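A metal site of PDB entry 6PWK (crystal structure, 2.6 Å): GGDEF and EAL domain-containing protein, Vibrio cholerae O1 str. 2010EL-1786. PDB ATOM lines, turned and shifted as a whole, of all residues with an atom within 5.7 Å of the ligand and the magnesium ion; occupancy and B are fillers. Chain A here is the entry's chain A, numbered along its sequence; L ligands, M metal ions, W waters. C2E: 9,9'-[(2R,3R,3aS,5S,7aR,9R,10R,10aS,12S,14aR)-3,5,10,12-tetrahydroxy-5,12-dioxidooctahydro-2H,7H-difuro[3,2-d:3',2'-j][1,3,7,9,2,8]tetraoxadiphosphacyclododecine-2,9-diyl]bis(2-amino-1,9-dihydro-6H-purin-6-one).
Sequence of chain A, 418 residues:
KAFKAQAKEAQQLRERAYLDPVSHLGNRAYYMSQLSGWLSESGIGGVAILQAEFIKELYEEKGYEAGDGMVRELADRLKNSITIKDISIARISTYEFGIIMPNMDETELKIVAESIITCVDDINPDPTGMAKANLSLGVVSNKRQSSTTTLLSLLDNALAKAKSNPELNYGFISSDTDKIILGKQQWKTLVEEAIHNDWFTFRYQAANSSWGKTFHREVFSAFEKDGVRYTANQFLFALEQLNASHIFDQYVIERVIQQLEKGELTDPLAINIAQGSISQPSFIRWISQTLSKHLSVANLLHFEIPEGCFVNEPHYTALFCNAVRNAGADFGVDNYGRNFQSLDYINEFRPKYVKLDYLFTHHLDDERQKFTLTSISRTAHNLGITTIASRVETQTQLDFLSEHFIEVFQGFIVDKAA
The magnesium ion is bound by O2P of the ligand (2.1 Å), OE1 of Glu 304 (2.2 Å), OD2 of Asp 334 (2.3 Å), OE2 of Glu 218 (2.3 Å), OD1 of Asn 272 (2.3 Å) and OD1 of Asp 334 (2.4 Å).
The backbone carbonyl oxygen (O) of Glu 304 is in hydrogen-bond range of the backbone NH (N) of Ile 273, at 3.0 Å. N of Glu 304 is in hydrogen-bond range of O of Ile 271, 2.7 Å away. The backbone carbonyl oxygen (O) of Asp 334 sits close to the backbone carbonyl oxygen (O) of Lys 355 (2.7 Å). ND2 of Asn 272 is in hydrogen-bond range of O of Val 219 (3.2 Å). The backbone carbonyl oxygen (O) of Arg 203 lies within hydrogen-bond range of the backbone NH (N) of Phe 220, at 2.9 Å. The side-chain carboxylate of Asp 249 lies within hydrogen-bond range of the backbone NH of Ala 274, 3.0 Å away. The backbone carbonyl oxygen (O) of Val 392 is in hydrogen-bond range of the backbone NH (N) of Phe 412 (3.1 Å). OE1 of Gln 205 sits at hydrogen-bond distance from NE2 of Gln 410.
The backbone carbonyl oxygen (O) of Asn 272 is in hydrogen-bond range of a nitrogen (N21) of the ligand (3.3 Å). A nitrogen (N2) of the ligand sits at hydrogen-bond distance from the side-chain carboxylate (OE1) of Glu 393. N of Ser 221 sits at hydrogen-bond distance from N71 of the ligand, at 3.2 Å. The side-chain hydroxyl of Ser 221 is in hydrogen-bond range of an oxygen (O61) of the ligand, 2.6 Å away. O21 of the ligand is in salt-bridge range of NH1 of Arg 203 (3.0 Å). The side-chain carboxylate of Asp 249 is in hydrogen-bond range of a nitrogen (N21) of the ligand. An oxygen (O1P) of the ligand is in salt-bridge range of the guanidinium group (NH1) of Arg 391 (2.7 Å). The backbone NH of Phe 412 lies within hydrogen-bond range of an oxygen (O6) of the ligand (2.8 Å). NE2 of Gln 205 is in hydrogen-bond range of N7 of the ligand (3.2 Å). The side-chain amide oxygen (OD1) of Asn 233 lies close to an oxygen (O4A) of the ligand (3.4 Å).
Water W1 lies within hydrogen-bond range of the backbone NH (N) of Asn 272 (2.7 Å), the backbone carbonyl oxygen (O) of Val 219 (2.7 Å) and an oxygen (O61) of the ligand (2.8 Å).
The backbone NH (N) of Ala 274 lies close to a nitrogen (N21) of the ligand (3.4 Å). An oxygen (O6) of the ligand sits close to the backbone carbonyl oxygen of Val 392 (3.4 Å). Phe 220 touches the ligand. CB of Thr 231 touches O11 of the ligand (3.9 Å). CB of Ala 232 touches O4A of the ligand, 3.2 Å away. Leu 236 touches the ligand (CD1 to N31, 3.5 Å). CE2 of Phe 248 touches N11 of the ligand (3.3 Å). Val 252 touches the ligand (CG1 to O61, 3.9 Å). Ile 273 touches the ligand. CA of Gly 411 touches O6 of the ligand, 3.3 Å away. Hydrophobic or aromatic side chains that line the ligand: Phe 220, Ala 232, Leu 236, Phe 248, Val 252 and Phe 412. Of the 30 residues printed, 21 come within 4 Å of the ligand.
The nearest printed residue that does not touch the magnesium ion is Lys 355 (4.8 Å).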
ATOM      1  N   ARG A 203     -18.545  -9.471  -8.235  1.00  0.00           N
ATOM      2  CA  ARG A 203     -19.670 -10.332  -8.551  1.00  0.00           C
ATOM      3  C   ARG A 203     -20.568 -10.477  -7.329  1.00  0.00           C
ATOM      4  O   ARG A 203     -20.072 -10.496  -6.191  1.00  0.00           O
ATOM      5  CB  ARG A 203     -19.196 -11.711  -9.018  1.00  0.00           C
ATOM      6  CG  ARG A 203     -18.450 -11.702 -10.346  1.00  0.00           C
ATOM      7  CD  ARG A 203     -17.656 -12.979 -10.577  1.00  0.00           C
ATOM      8  NE  ARG A 203     -18.376 -14.173 -10.122  1.00  0.00           N
ATOM      9  CZ  ARG A 203     -17.886 -15.032  -9.236  1.00  0.00           C
ATOM     10  NH1 ARG A 203     -16.681 -14.842  -8.714  1.00  0.00           N
ATOM     11  NH2 ARG A 203     -18.598 -16.095  -8.880  1.00  0.00           N
ATOM     12  N   GLN A 205     -23.505 -12.875  -5.782  1.00  0.00           N
ATOM     13  CA  GLN A 205     -24.230 -14.134  -5.823  1.00  0.00           C
ATOM     14  C   GLN A 205     -25.286 -14.143  -4.719  1.00  0.00           C
ATOM     15  O   GLN A 205     -24.947 -13.990  -3.542  1.00  0.00           O
ATOM     16  CB  GLN A 205     -23.288 -15.331  -5.676  1.00  0.00           C
ATOM     17  CG  GLN A 205     -23.939 -16.667  -5.990  1.00  0.00           C
ATOM     18  CD  GLN A 205     -23.000 -17.836  -5.806  1.00  0.00           C
ATOM     19  OE1 GLN A 205     -22.298 -17.945  -4.803  1.00  0.00           O
ATOM     20  NE2 GLN A 205     -22.970 -18.730  -6.792  1.00  0.00           N
ATOM     21  N   GLU A 218     -23.634 -12.330  -1.636  1.00  0.00           N
ATOM     22  CA  GLU A 218     -22.232 -12.389  -1.287  1.00  0.00           C
ATOM     23  C   GLU A 218     -21.383 -11.734  -2.369  1.00  0.00           C
ATOM     24  O   GLU A 218     -21.617 -11.920  -3.562  1.00  0.00           O
ATOM     25  CB  GLU A 218     -21.781 -13.841  -1.079  1.00  0.00           C
ATOM     26  CG  GLU A 218     -20.328 -13.976  -0.662  1.00  0.00           C
ATOM     27  CD  GLU A 218     -19.952 -15.399  -0.289  1.00  0.00           C
ATOM     28  OE1 GLU A 218     -20.793 -16.306  -0.468  1.00  0.00           O
ATOM     29  OE2 GLU A 218     -18.816 -15.611   0.177  1.00  0.00           O
ATOM     30  N   VAL A 219     -20.388 -10.957  -1.936  1.00  0.00           N
ATOM     31  CA  VAL A 219     -19.524 -10.201  -2.835  1.00  0.00           C
ATOM     32  C   VAL A 219     -18.245 -10.986  -3.068  1.00  0.00           C
ATOM     33  O   VAL A 219     -17.576 -11.409  -2.112  1.00  0.00           O
ATOM     34  CB  VAL A 219     -19.227  -8.803  -2.273  1.00  0.00           C
ATOM     35  CG1 VAL A 219     -18.239  -8.072  -3.164  1.00  0.00           C
ATOM     36  CG2 VAL A 219     -20.513  -8.014  -2.107  1.00  0.00           C
ATOM     37  N   PHE A 220     -17.896 -11.193  -4.341  1.00  0.00           N
ATOM     38  CA  PHE A 220     -16.654 -11.832  -4.730  1.00  0.00           C
ATOM     39  C   PHE A 220     -15.785 -10.827  -5.466  1.00  0.00           C
ATOM     40  O   PHE A 220     -16.250 -10.155  -6.391  1.00  0.00           O
ATOM     41  CB  PHE A 220     -16.921 -13.051  -5.625  1.00  0.00           C
ATOM     42  CG  PHE A 220     -17.663 -14.145  -4.926  1.00  0.00           C
ATOM     43  CD1 PHE A 220     -17.362 -14.497  -3.629  1.00  0.00           C
ATOM     44  CD2 PHE A 220     -18.690 -14.822  -5.567  1.00  0.00           C
ATOM     45  CE1 PHE A 220     -18.049 -15.498  -2.976  1.00  0.00           C
ATOM     46  CE2 PHE A 220     -19.393 -15.828  -4.930  1.00  0.00           C
ATOM     47  CZ  PHE A 220     -19.068 -16.163  -3.637  1.00  0.00           C
ATOM     48  N   SER A 221     -14.524 -10.724  -5.045  1.00  0.00           N
ATOM     49  CA  SER A 221     -13.608  -9.734  -5.599  1.00  0.00           C
ATOM     50  C   SER A 221     -12.625 -10.388  -6.555  1.00  0.00           C
ATOM     51  O   SER A 221     -12.132 -11.486  -6.307  1.00  0.00           O
ATOM     52  CB  SER A 221     -12.843  -9.024  -4.471  1.00  0.00           C
ATOM     53  OG  SER A 221     -13.736  -8.336  -3.608  1.00  0.00           O
ATOM     54  N   THR A 231      -8.290 -14.086  -9.397  1.00  0.00           N
ATOM     55  CA  THR A 231      -9.271 -14.290  -8.336  1.00  0.00           C
ATOM     56  C   THR A 231      -8.581 -14.338  -6.976  1.00  0.00           C
ATOM     57  O   THR A 231      -7.358 -14.404  -6.874  1.00  0.00           O
ATOM     58  CB  THR A 231     -10.088 -15.559  -8.578  1.00  0.00           C
ATOM     59  OG1 THR A 231      -9.241 -16.714  -8.467  1.00  0.00           O
ATOM     60  CG2 THR A 231     -10.716 -15.532  -9.965  1.00  0.00           C
ATOM     61  N   ALA A 232      -9.404 -14.313  -5.918  1.00  0.00           N
ATOM     62  CA  ALA A 232      -8.879 -14.072  -4.583  1.00  0.00           C
ATOM     63  C   ALA A 232      -8.009 -15.224  -4.084  1.00  0.00           C
ATOM     64  O   ALA A 232      -7.003 -14.988  -3.400  1.00  0.00           O
ATOM     65  CB  ALA A 232     -10.040 -13.815  -3.610  1.00  0.00           C
ATOM     66  N   ASN A 233      -8.369 -16.464  -4.410  1.00  0.00           N
ATOM     67  CA  ASN A 233      -7.581 -17.600  -3.953  1.00  0.00           C
ATOM     68  C   ASN A 233      -6.203 -17.674  -4.591  1.00  0.00           C
ATOM     69  O   ASN A 233      -5.397 -18.520  -4.196  1.00  0.00           O
ATOM     70  CB  ASN A 233      -8.337 -18.914  -4.201  1.00  0.00           C
ATOM     71  CG  ASN A 233      -9.356 -19.211  -3.113  1.00  0.00           C
ATOM     72  OD1 ASN A 233      -9.288 -18.659  -2.020  1.00  0.00           O
ATOM     73  ND2 ASN A 233     -10.292 -20.110  -3.407  1.00  0.00           N
ATOM     74  N   LEU A 236      -4.544 -14.446  -1.923  1.00  0.00           N
ATOM     75  CA  LEU A 236      -4.880 -14.206  -0.520  1.00  0.00           C
ATOM     76  C   LEU A 236      -3.862 -14.838   0.427  1.00  0.00           C
ATOM     77  O   LEU A 236      -3.660 -14.328   1.542  1.00  0.00           O
ATOM     78  CB  LEU A 236      -6.273 -14.725  -0.205  1.00  0.00           C
ATOM     79  CG  LEU A 236      -7.404 -13.703  -0.360  1.00  0.00           C
ATOM     80  CD1 LEU A 236      -8.754 -14.345  -0.082  1.00  0.00           C
ATOM     81  CD2 LEU A 236      -7.170 -12.513   0.558  1.00  0.00           C
ATOM     82  N   PHE A 248      -6.418  -5.176   1.673  1.00  0.00           N
ATOM     83  CA  PHE A 248      -7.348  -5.658   0.656  1.00  0.00           C
ATOM     84  C   PHE A 248      -8.787  -5.641   1.169  1.00  0.00           C
ATOM     85  O   PHE A 248      -9.701  -5.241   0.431  1.00  0.00           O
ATOM     86  CB  PHE A 248      -6.936  -7.068   0.224  1.00  0.00           C
ATOM     87  CG  PHE A 248      -7.966  -7.784  -0.583  1.00  0.00           C
ATOM     88  CD1 PHE A 248      -8.154  -7.481  -1.927  1.00  0.00           C
ATOM     89  CD2 PHE A 248      -8.748  -8.775  -0.012  1.00  0.00           C
ATOM     90  CE1 PHE A 248      -9.109  -8.147  -2.669  1.00  0.00           C
ATOM     91  CE2 PHE A 248      -9.694  -9.443  -0.756  1.00  0.00           C
ATOM     92  CZ  PHE A 248      -9.876  -9.133  -2.083  1.00  0.00           C
ATOM     93  N   ASP A 249      -9.000  -6.052   2.413  1.00  0.00           N
ATOM     94  CA  ASP A 249     -10.356  -6.078   2.956  1.00  0.00           C
ATOM     95  C   ASP A 249     -10.910  -4.667   3.146  1.00  0.00           C
ATOM     96  O   ASP A 249     -12.104  -4.433   2.910  1.00  0.00           O
ATOM     97  CB  ASP A 249     -10.385  -6.845   4.279  1.00  0.00           C
ATOM     98  CG  ASP A 249     -10.445  -8.345   4.086  1.00  0.00           C
ATOM     99  OD1 ASP A 249     -10.879  -8.786   3.000  1.00  0.00           O
ATOM    100  OD2 ASP A 249     -10.053  -9.085   5.009  1.00  0.00           O
ATOM    101  N   VAL A 252     -12.113  -3.453  -0.281  1.00  0.00           N
ATOM    102  CA  VAL A 252     -13.371  -4.088  -0.679  1.00  0.00           C
ATOM    103  C   VAL A 252     -14.537  -3.502   0.112  1.00  0.00           C
ATOM    104  O   VAL A 252     -15.600  -3.200  -0.451  1.00  0.00           O
ATOM    105  CB  VAL A 252     -13.283  -5.614  -0.508  1.00  0.00           C
ATOM    106  CG1 VAL A 252     -14.637  -6.260  -0.740  1.00  0.00           C
ATOM    107  CG2 VAL A 252     -12.236  -6.189  -1.463  1.00  0.00           C
ATOM    108  N   ILE A 271     -19.844  -9.555   2.871  1.00  0.00           N
ATOM    109  CA  ILE A 271     -18.450  -9.268   2.554  1.00  0.00           C
ATOM    110  C   ILE A 271     -17.570 -10.303   3.244  1.00  0.00           C
ATOM    111  O   ILE A 271     -17.653 -10.489   4.465  1.00  0.00           O
ATOM    112  CB  ILE A 271     -18.060  -7.845   3.003  1.00  0.00           C
ATOM    113  CG1 ILE A 271     -19.003  -6.809   2.394  1.00  0.00           C
ATOM    114  CG2 ILE A 271     -16.618  -7.551   2.620  1.00  0.00           C
ATOM    115  CD1 ILE A 271     -18.687  -5.397   2.819  1.00  0.00           C
ATOM    116  N   ASN A 272     -16.726 -10.980   2.465  1.00  0.00           N
ATOM    117  CA  ASN A 272     -15.779 -11.923   3.036  1.00  0.00           C
ATOM    118  C   ASN A 272     -14.636 -11.178   3.720  1.00  0.00           C
ATOM    119  O   ASN A 272     -14.145 -10.155   3.226  1.00  0.00           O
ATOM    120  CB  ASN A 272     -15.212 -12.838   1.954  1.00  0.00           C
ATOM    121  CG  ASN A 272     -16.249 -13.774   1.371  1.00  0.00           C
ATOM    122  OD1 ASN A 272     -16.626 -14.773   1.983  1.00  0.00           O
ATOM    123  ND2 ASN A 272     -16.717 -13.459   0.164  1.00  0.00           N
ATOM    124  N   ILE A 273     -14.205 -11.691   4.870  1.00  0.00           N
ATOM    125  CA  ILE A 273     -13.100 -11.128   5.629  1.00  0.00           C
ATOM    126  C   ILE A 273     -12.074 -12.221   5.863  1.00  0.00           C
ATOM    127  O   ILE A 273     -12.416 -13.320   6.307  1.00  0.00           O
ATOM    128  CB  ILE A 273     -13.571 -10.537   6.982  1.00  0.00           C
ATOM    129  CG1 ILE A 273     -14.699  -9.528   6.773  1.00  0.00           C
ATOM    130  CG2 ILE A 273     -12.403  -9.907   7.713  1.00  0.00           C
ATOM    131  CD1 ILE A 273     -14.283  -8.289   5.996  1.00  0.00           C
ATOM    132  N   ALA A 274     -10.820 -11.936   5.544  1.00  0.00           N
ATOM    133  CA  ALA A 274      -9.758 -12.900   5.783  1.00  0.00           C
ATOM    134  C   ALA A 274      -9.401 -12.957   7.263  1.00  0.00           C
ATOM    135  O   ALA A 274      -9.666 -12.027   8.030  1.00  0.00           O
ATOM    136  CB  ALA A 274      -8.513 -12.554   4.954  1.00  0.00           C
ATOM    137  N   GLU A 304     -18.780 -11.851   6.498  1.00  0.00           N
ATOM    138  CA  GLU A 304     -18.602 -13.298   6.455  1.00  0.00           C
ATOM    139  C   GLU A 304     -17.234 -13.638   7.030  1.00  0.00           C
ATOM    140  O   GLU A 304     -16.202 -13.324   6.431  1.00  0.00           O
ATOM    141  CB  GLU A 304     -18.754 -13.810   5.026  1.00  0.00           C
ATOM    142  CG  GLU A 304     -19.290 -15.237   4.943  1.00  0.00           C
ATOM    143  CD  GLU A 304     -20.122 -15.474   3.691  1.00  0.00           C
ATOM    144  OE1 GLU A 304     -19.570 -15.965   2.689  1.00  0.00           O
ATOM    145  OE2 GLU A 304     -21.330 -15.166   3.717  1.00  0.00           O
ATOM    146  N   ASP A 334     -18.414 -18.684   7.584  1.00  0.00           N
ATOM    147  CA  ASP A 334     -18.211 -19.008   6.173  1.00  0.00           C
ATOM    148  C   ASP A 334     -17.929 -20.495   5.924  1.00  0.00           C
ATOM    149  O   ASP A 334     -18.569 -21.110   5.075  1.00  0.00           O
ATOM    150  CB  ASP A 334     -17.067 -18.155   5.607  1.00  0.00           C
ATOM    151  CG  ASP A 334     -17.165 -17.984   4.097  1.00  0.00           C
ATOM    152  OD1 ASP A 334     -18.097 -18.539   3.486  1.00  0.00           O
ATOM    153  OD2 ASP A 334     -16.313 -17.263   3.536  1.00  0.00           O
ATOM    154  N   ASN A 335     -16.971 -21.074   6.646  1.00  0.00           N
ATOM    155  CA  ASN A 335     -16.645 -22.493   6.490  1.00  0.00           C
ATOM    156  C   ASN A 335     -17.319 -23.349   7.549  1.00  0.00           C
ATOM    157  O   ASN A 335     -16.707 -24.237   8.136  1.00  0.00           O
ATOM    158  CB  ASN A 335     -15.130 -22.698   6.545  1.00  0.00           C
ATOM    159  CG  ASN A 335     -14.440 -22.238   5.270  1.00  0.00           C
ATOM    160  OD1 ASN A 335     -15.036 -22.254   4.195  1.00  0.00           O
ATOM    161  ND2 ASN A 335     -13.182 -21.836   5.393  1.00  0.00           N
ATOM    162  N   LYS A 355     -23.022 -20.298   6.894  1.00  0.00           N
ATOM    163  CA  LYS A 355     -22.900 -20.778   5.530  1.00  0.00           C
ATOM    164  C   LYS A 355     -22.105 -22.073   5.555  1.00  0.00           C
ATOM    165  O   LYS A 355     -20.941 -22.082   5.965  1.00  0.00           O
ATOM    166  CB  LYS A 355     -22.236 -19.734   4.641  1.00  0.00           C
ATOM    167  CG  LYS A 355     -22.430 -19.973   3.145  1.00  0.00           C
ATOM    168  CD  LYS A 355     -22.095 -18.724   2.338  1.00  0.00           C
ATOM    169  CE  LYS A 355     -22.990 -17.559   2.731  1.00  0.00           C
ATOM    170  NZ  LYS A 355     -22.734 -16.361   1.883  1.00  0.00           N
ATOM    171  N   TYR A 358     -18.529 -25.905   1.815  1.00  0.00           N
ATOM    172  CA  TYR A 358     -18.899 -26.374   0.487  1.00  0.00           C
ATOM    173  C   TYR A 358     -18.532 -27.834   0.252  1.00  0.00           C
ATOM    174  O   TYR A 358     -18.986 -28.408  -0.741  1.00  0.00           O
ATOM    175  CB  TYR A 358     -18.243 -25.489  -0.587  1.00  0.00           C
ATOM    176  CG  TYR A 358     -16.778 -25.758  -0.841  1.00  0.00           C
ATOM    177  CD1 TYR A 358     -15.795 -25.124  -0.086  1.00  0.00           C
ATOM    178  CD2 TYR A 358     -16.371 -26.613  -1.862  1.00  0.00           C
ATOM    179  CE1 TYR A 358     -14.445 -25.352  -0.334  1.00  0.00           C
ATOM    180  CE2 TYR A 358     -15.032 -26.847  -2.104  1.00  0.00           C
ATOM    181  CZ  TYR A 358     -14.079 -26.215  -1.337  1.00  0.00           C
ATOM    182  OH  TYR A 358     -12.743 -26.453  -1.587  1.00  0.00           O
ATOM    183  N   SER A 390     -23.873 -23.923   0.560  1.00  0.00           N
ATOM    184  CA  SER A 390     -22.857 -23.191  -0.194  1.00  0.00           C
ATOM    185  C   SER A 390     -22.426 -23.975  -1.423  1.00  0.00           C
ATOM    186  O   SER A 390     -22.233 -25.192  -1.367  1.00  0.00           O
ATOM    187  CB  SER A 390     -21.639 -22.896   0.693  1.00  0.00           C
ATOM    188  OG  SER A 390     -20.628 -22.215  -0.028  1.00  0.00           O
ATOM    189  N   ARG A 391     -22.271 -23.242  -2.531  1.00  0.00           N
ATOM    190  CA  ARG A 391     -21.701 -23.776  -3.773  1.00  0.00           C
ATOM    191  C   ARG A 391     -22.513 -24.957  -4.313  1.00  0.00           C
ATOM    192  O   ARG A 391     -21.965 -25.998  -4.690  1.00  0.00           O
ATOM    193  CB  ARG A 391     -20.220 -24.144  -3.573  1.00  0.00           C
ATOM    194  CG  ARG A 391     -19.296 -22.945  -3.801  1.00  0.00           C
ATOM    195  CD  ARG A 391     -18.179 -22.807  -2.780  1.00  0.00           C
ATOM    196  NE  ARG A 391     -16.958 -23.491  -3.201  1.00  0.00           N
ATOM    197  CZ  ARG A 391     -15.726 -23.098  -2.858  1.00  0.00           C
ATOM    198  NH1 ARG A 391     -15.559 -22.018  -2.111  1.00  0.00           N
ATOM    199  NH2 ARG A 391     -14.675 -23.771  -3.286  1.00  0.00           N
ATOM    200  N   VAL A 392     -23.828 -24.775  -4.356  1.00  0.00           N
ATOM    201  CA  VAL A 392     -24.731 -25.793  -4.879  1.00  0.00           C
ATOM    202  C   VAL A 392     -24.755 -25.692  -6.402  1.00  0.00           C
ATOM    203  O   VAL A 392     -25.101 -24.643  -6.961  1.00  0.00           O
ATOM    204  CB  VAL A 392     -26.142 -25.619  -4.302  1.00  0.00           C
ATOM    205  CG1 VAL A 392     -26.998 -26.838  -4.616  1.00  0.00           C
ATOM    206  CG2 VAL A 392     -26.075 -25.373  -2.805  1.00  0.00           C
ATOM    207  N   GLU A 393     -24.377 -26.782  -7.070  1.00  0.00           N
ATOM    208  CA  GLU A 393     -24.259 -26.826  -8.523  1.00  0.00           C
ATOM    209  C   GLU A 393     -25.366 -27.590  -9.213  1.00  0.00           C
ATOM    210  O   GLU A 393     -25.783 -27.200 -10.310  1.00  0.00           O
ATOM    211  CB  GLU A 393     -22.913 -27.456  -8.932  1.00  0.00           C
ATOM    212  CG  GLU A 393     -21.693 -26.750  -8.434  1.00  0.00           C
ATOM    213  CD  GLU A 393     -20.427 -27.251  -9.102  1.00  0.00           C
ATOM    214  OE1 GLU A 393     -19.712 -26.444  -9.736  1.00  0.00           O
ATOM    215  OE2 GLU A 393     -20.149 -28.465  -9.011  1.00  0.00           O
ATOM    216  N   GLN A 410     -27.255 -21.253  -2.012  1.00  0.00           N
ATOM    217  CA  GLN A 410     -26.402 -20.390  -2.823  1.00  0.00           C
ATOM    218  C   GLN A 410     -25.565 -21.246  -3.759  1.00  0.00           C
ATOM    219  O   GLN A 410     -25.116 -22.332  -3.373  1.00  0.00           O
ATOM    220  CB  GLN A 410     -25.500 -19.511  -1.939  1.00  0.00           C
ATOM    221  CG  GLN A 410     -24.707 -18.456  -2.687  1.00  0.00           C
ATOM    222  CD  GLN A 410     -23.844 -17.600  -1.768  1.00  0.00           C
ATOM    223  OE1 GLN A 410     -23.968 -17.658  -0.546  1.00  0.00           O
ATOM    224  NE2 GLN A 410     -22.950 -16.811  -2.360  1.00  0.00           N
ATOM    225  N   GLY A 411     -25.358 -20.775  -4.967  1.00  0.00           N
ATOM    226  CA  GLY A 411     -24.557 -21.504  -5.926  1.00  0.00           C
ATOM    227  C   GLY A 411     -25.021 -21.229  -7.348  1.00  0.00           C
ATOM    228  O   GLY A 411     -25.927 -20.434  -7.592  1.00  0.00           O
ATOM    229  N   PHE A 412     -24.380 -21.937  -8.288  1.00  0.00           N
ATOM    230  CA  PHE A 412     -24.663 -21.717  -9.700  1.00  0.00           C
ATOM    231  C   PHE A 412     -26.032 -22.247 -10.096  1.00  0.00           C
ATOM    232  O   PHE A 412     -26.635 -21.735 -11.054  1.00  0.00           O
ATOM    233  CB  PHE A 412     -23.566 -22.375 -10.550  1.00  0.00           C
ATOM    234  CG  PHE A 412     -22.216 -21.734 -10.407  1.00  0.00           C
ATOM    235  CD1 PHE A 412     -22.101 -20.393 -10.059  1.00  0.00           C
ATOM    236  CD2 PHE A 412     -21.061 -22.462 -10.602  1.00  0.00           C
ATOM    237  CE1 PHE A 412     -20.862 -19.795  -9.924  1.00  0.00           C
ATOM    238  CE2 PHE A 412     -19.813 -21.867 -10.470  1.00  0.00           C
ATOM    239  CZ  PHE A 412     -19.712 -20.536 -10.125  1.00  0.00           C
ATOM    240  N   ILE A 413     -26.546 -23.252  -9.395  1.00  0.00           N
ATOM    241  CA  ILE A 413     -27.866 -23.783  -9.729  1.00  0.00           C
ATOM    242  C   ILE A 413     -28.982 -22.851  -9.286  1.00  0.00           C
ATOM    243  O   ILE A 413     -30.072 -22.871  -9.861  1.00  0.00           O
ATOM    244  CB  ILE A 413     -28.067 -25.182  -9.143  1.00  0.00           C
ATOM    245  CG1 ILE A 413     -29.199 -25.900  -9.888  1.00  0.00           C
ATOM    246  CG2 ILE A 413     -28.350 -25.117  -7.647  1.00  0.00           C
ATOM    247  CD1 ILE A 413     -29.947 -26.914  -9.059  1.00  0.00           C
HETATM  248  P1  C2E L   1     -15.862 -18.485  -0.688  1.00  0.00           P
HETATM  249  O2P C2E L   1     -16.366 -17.768   0.539  1.00  0.00           O
HETATM  250  O1P C2E L   1     -16.202 -19.930  -0.475  1.00  0.00           O
HETATM  251  O5' C2E L   1     -16.700 -18.052  -2.026  1.00  0.00           O
HETATM  252  C5' C2E L   1     -17.263 -19.063  -2.796  1.00  0.00           C
HETATM  253  C4' C2E L   1     -16.255 -19.336  -3.955  1.00  0.00           C
HETATM  254  O4' C2E L   1     -16.663 -20.346  -4.671  1.00  0.00           O
HETATM  255  C3' C2E L   1     -16.245 -18.172  -4.958  1.00  0.00           C
HETATM  256  O3' C2E L   1     -15.156 -18.342  -5.732  1.00  0.00           O
HETATM  257  C2' C2E L   1     -17.481 -18.500  -5.802  1.00  0.00           C
HETATM  258  O2' C2E L   1     -17.437 -17.753  -7.089  1.00  0.00           O
HETATM  259  C1' C2E L   1     -17.236 -19.753  -6.059  1.00  0.00           C
HETATM  260  N9  C2E L   1     -18.299 -20.662  -6.415  1.00  0.00           N
HETATM  261  C8  C2E L   1     -19.367 -19.913  -6.044  1.00  0.00           C
HETATM  262  N7  C2E L   1     -20.477 -20.653  -6.310  1.00  0.00           N
HETATM  263  C5  C2E L   1     -20.098 -21.819  -6.824  1.00  0.00           C
HETATM  264  C6  C2E L   1     -20.850 -23.065  -7.316  1.00  0.00           C
HETATM  265  O6  C2E L   1     -22.030 -23.127  -7.294  1.00  0.00           O
HETATM  266  N1  C2E L   1     -20.111 -24.187  -7.814  1.00  0.00           N
HETATM  267  C2  C2E L   1     -18.672 -24.173  -7.860  1.00  0.00           C
HETATM  268  N2  C2E L   1     -17.870 -25.295  -8.360  1.00  0.00           N
HETATM  269  N3  C2E L   1     -17.995 -22.989  -7.384  1.00  0.00           N
HETATM  270  C4  C2E L   1     -18.746 -21.813  -6.867  1.00  0.00           C
HETATM  271  P11 C2E L   1     -14.214 -16.975  -5.827  1.00  0.00           P
HETATM  272  O21 C2E L   1     -14.769 -15.779  -6.545  1.00  0.00           O
HETATM  273  O11 C2E L   1     -12.985 -17.370  -6.614  1.00  0.00           O
HETATM  274  O5A C2E L   1     -13.790 -16.766  -4.248  1.00  0.00           O
HETATM  275  C5A C2E L   1     -12.848 -17.703  -3.813  1.00  0.00           C
HETATM  276  C4A C2E L   1     -12.421 -17.395  -2.433  1.00  0.00           C
HETATM  277  O4A C2E L   1     -11.734 -16.287  -2.421  1.00  0.00           O
HETATM  278  C3A C2E L   1     -13.767 -17.161  -1.448  1.00  0.00           C
HETATM  279  O3A C2E L   1     -14.208 -18.466  -0.852  1.00  0.00           O
HETATM  280  C2A C2E L   1     -13.399 -16.393  -0.566  1.00  0.00           C
HETATM  281  O2A C2E L   1     -12.834 -17.175   0.591  1.00  0.00           O
HETATM  282  C1A C2E L   1     -12.252 -15.476  -1.260  1.00  0.00           C
HETATM  283  N91 C2E L   1     -12.763 -14.331  -1.656  1.00  0.00           N
HETATM  284  C81 C2E L   1     -13.468 -14.046  -2.761  1.00  0.00           C
HETATM  285  N71 C2E L   1     -13.750 -12.729  -2.696  1.00  0.00           N
HETATM  286  C51 C2E L   1     -13.228 -12.239  -1.571  1.00  0.00           C
HETATM  287  C61 C2E L   1     -13.231 -10.838  -0.974  1.00  0.00           C
HETATM  288  O61 C2E L   1     -13.782  -9.968  -1.556  1.00  0.00           O
HETATM  289  N11 C2E L   1     -12.583 -10.573   0.281  1.00  0.00           N
HETATM  290  C21 C2E L   1     -11.919 -11.628   0.981  1.00  0.00           C
HETATM  291  N21 C2E L   1     -11.268 -11.360   2.245  1.00  0.00           N
HETATM  292  N31 C2E L   1     -11.931 -12.970   0.390  1.00  0.00           N
HETATM  293  C41 C2E L   1     -12.604 -13.239  -0.910  1.00  0.00           C
HETATM  294 MG    MG M   1     -17.754 -16.790   1.844  1.00  0.00          MG
HETATM  295  O   HOH W   1     -16.148 -10.344  -0.067  1.00  0.00           O
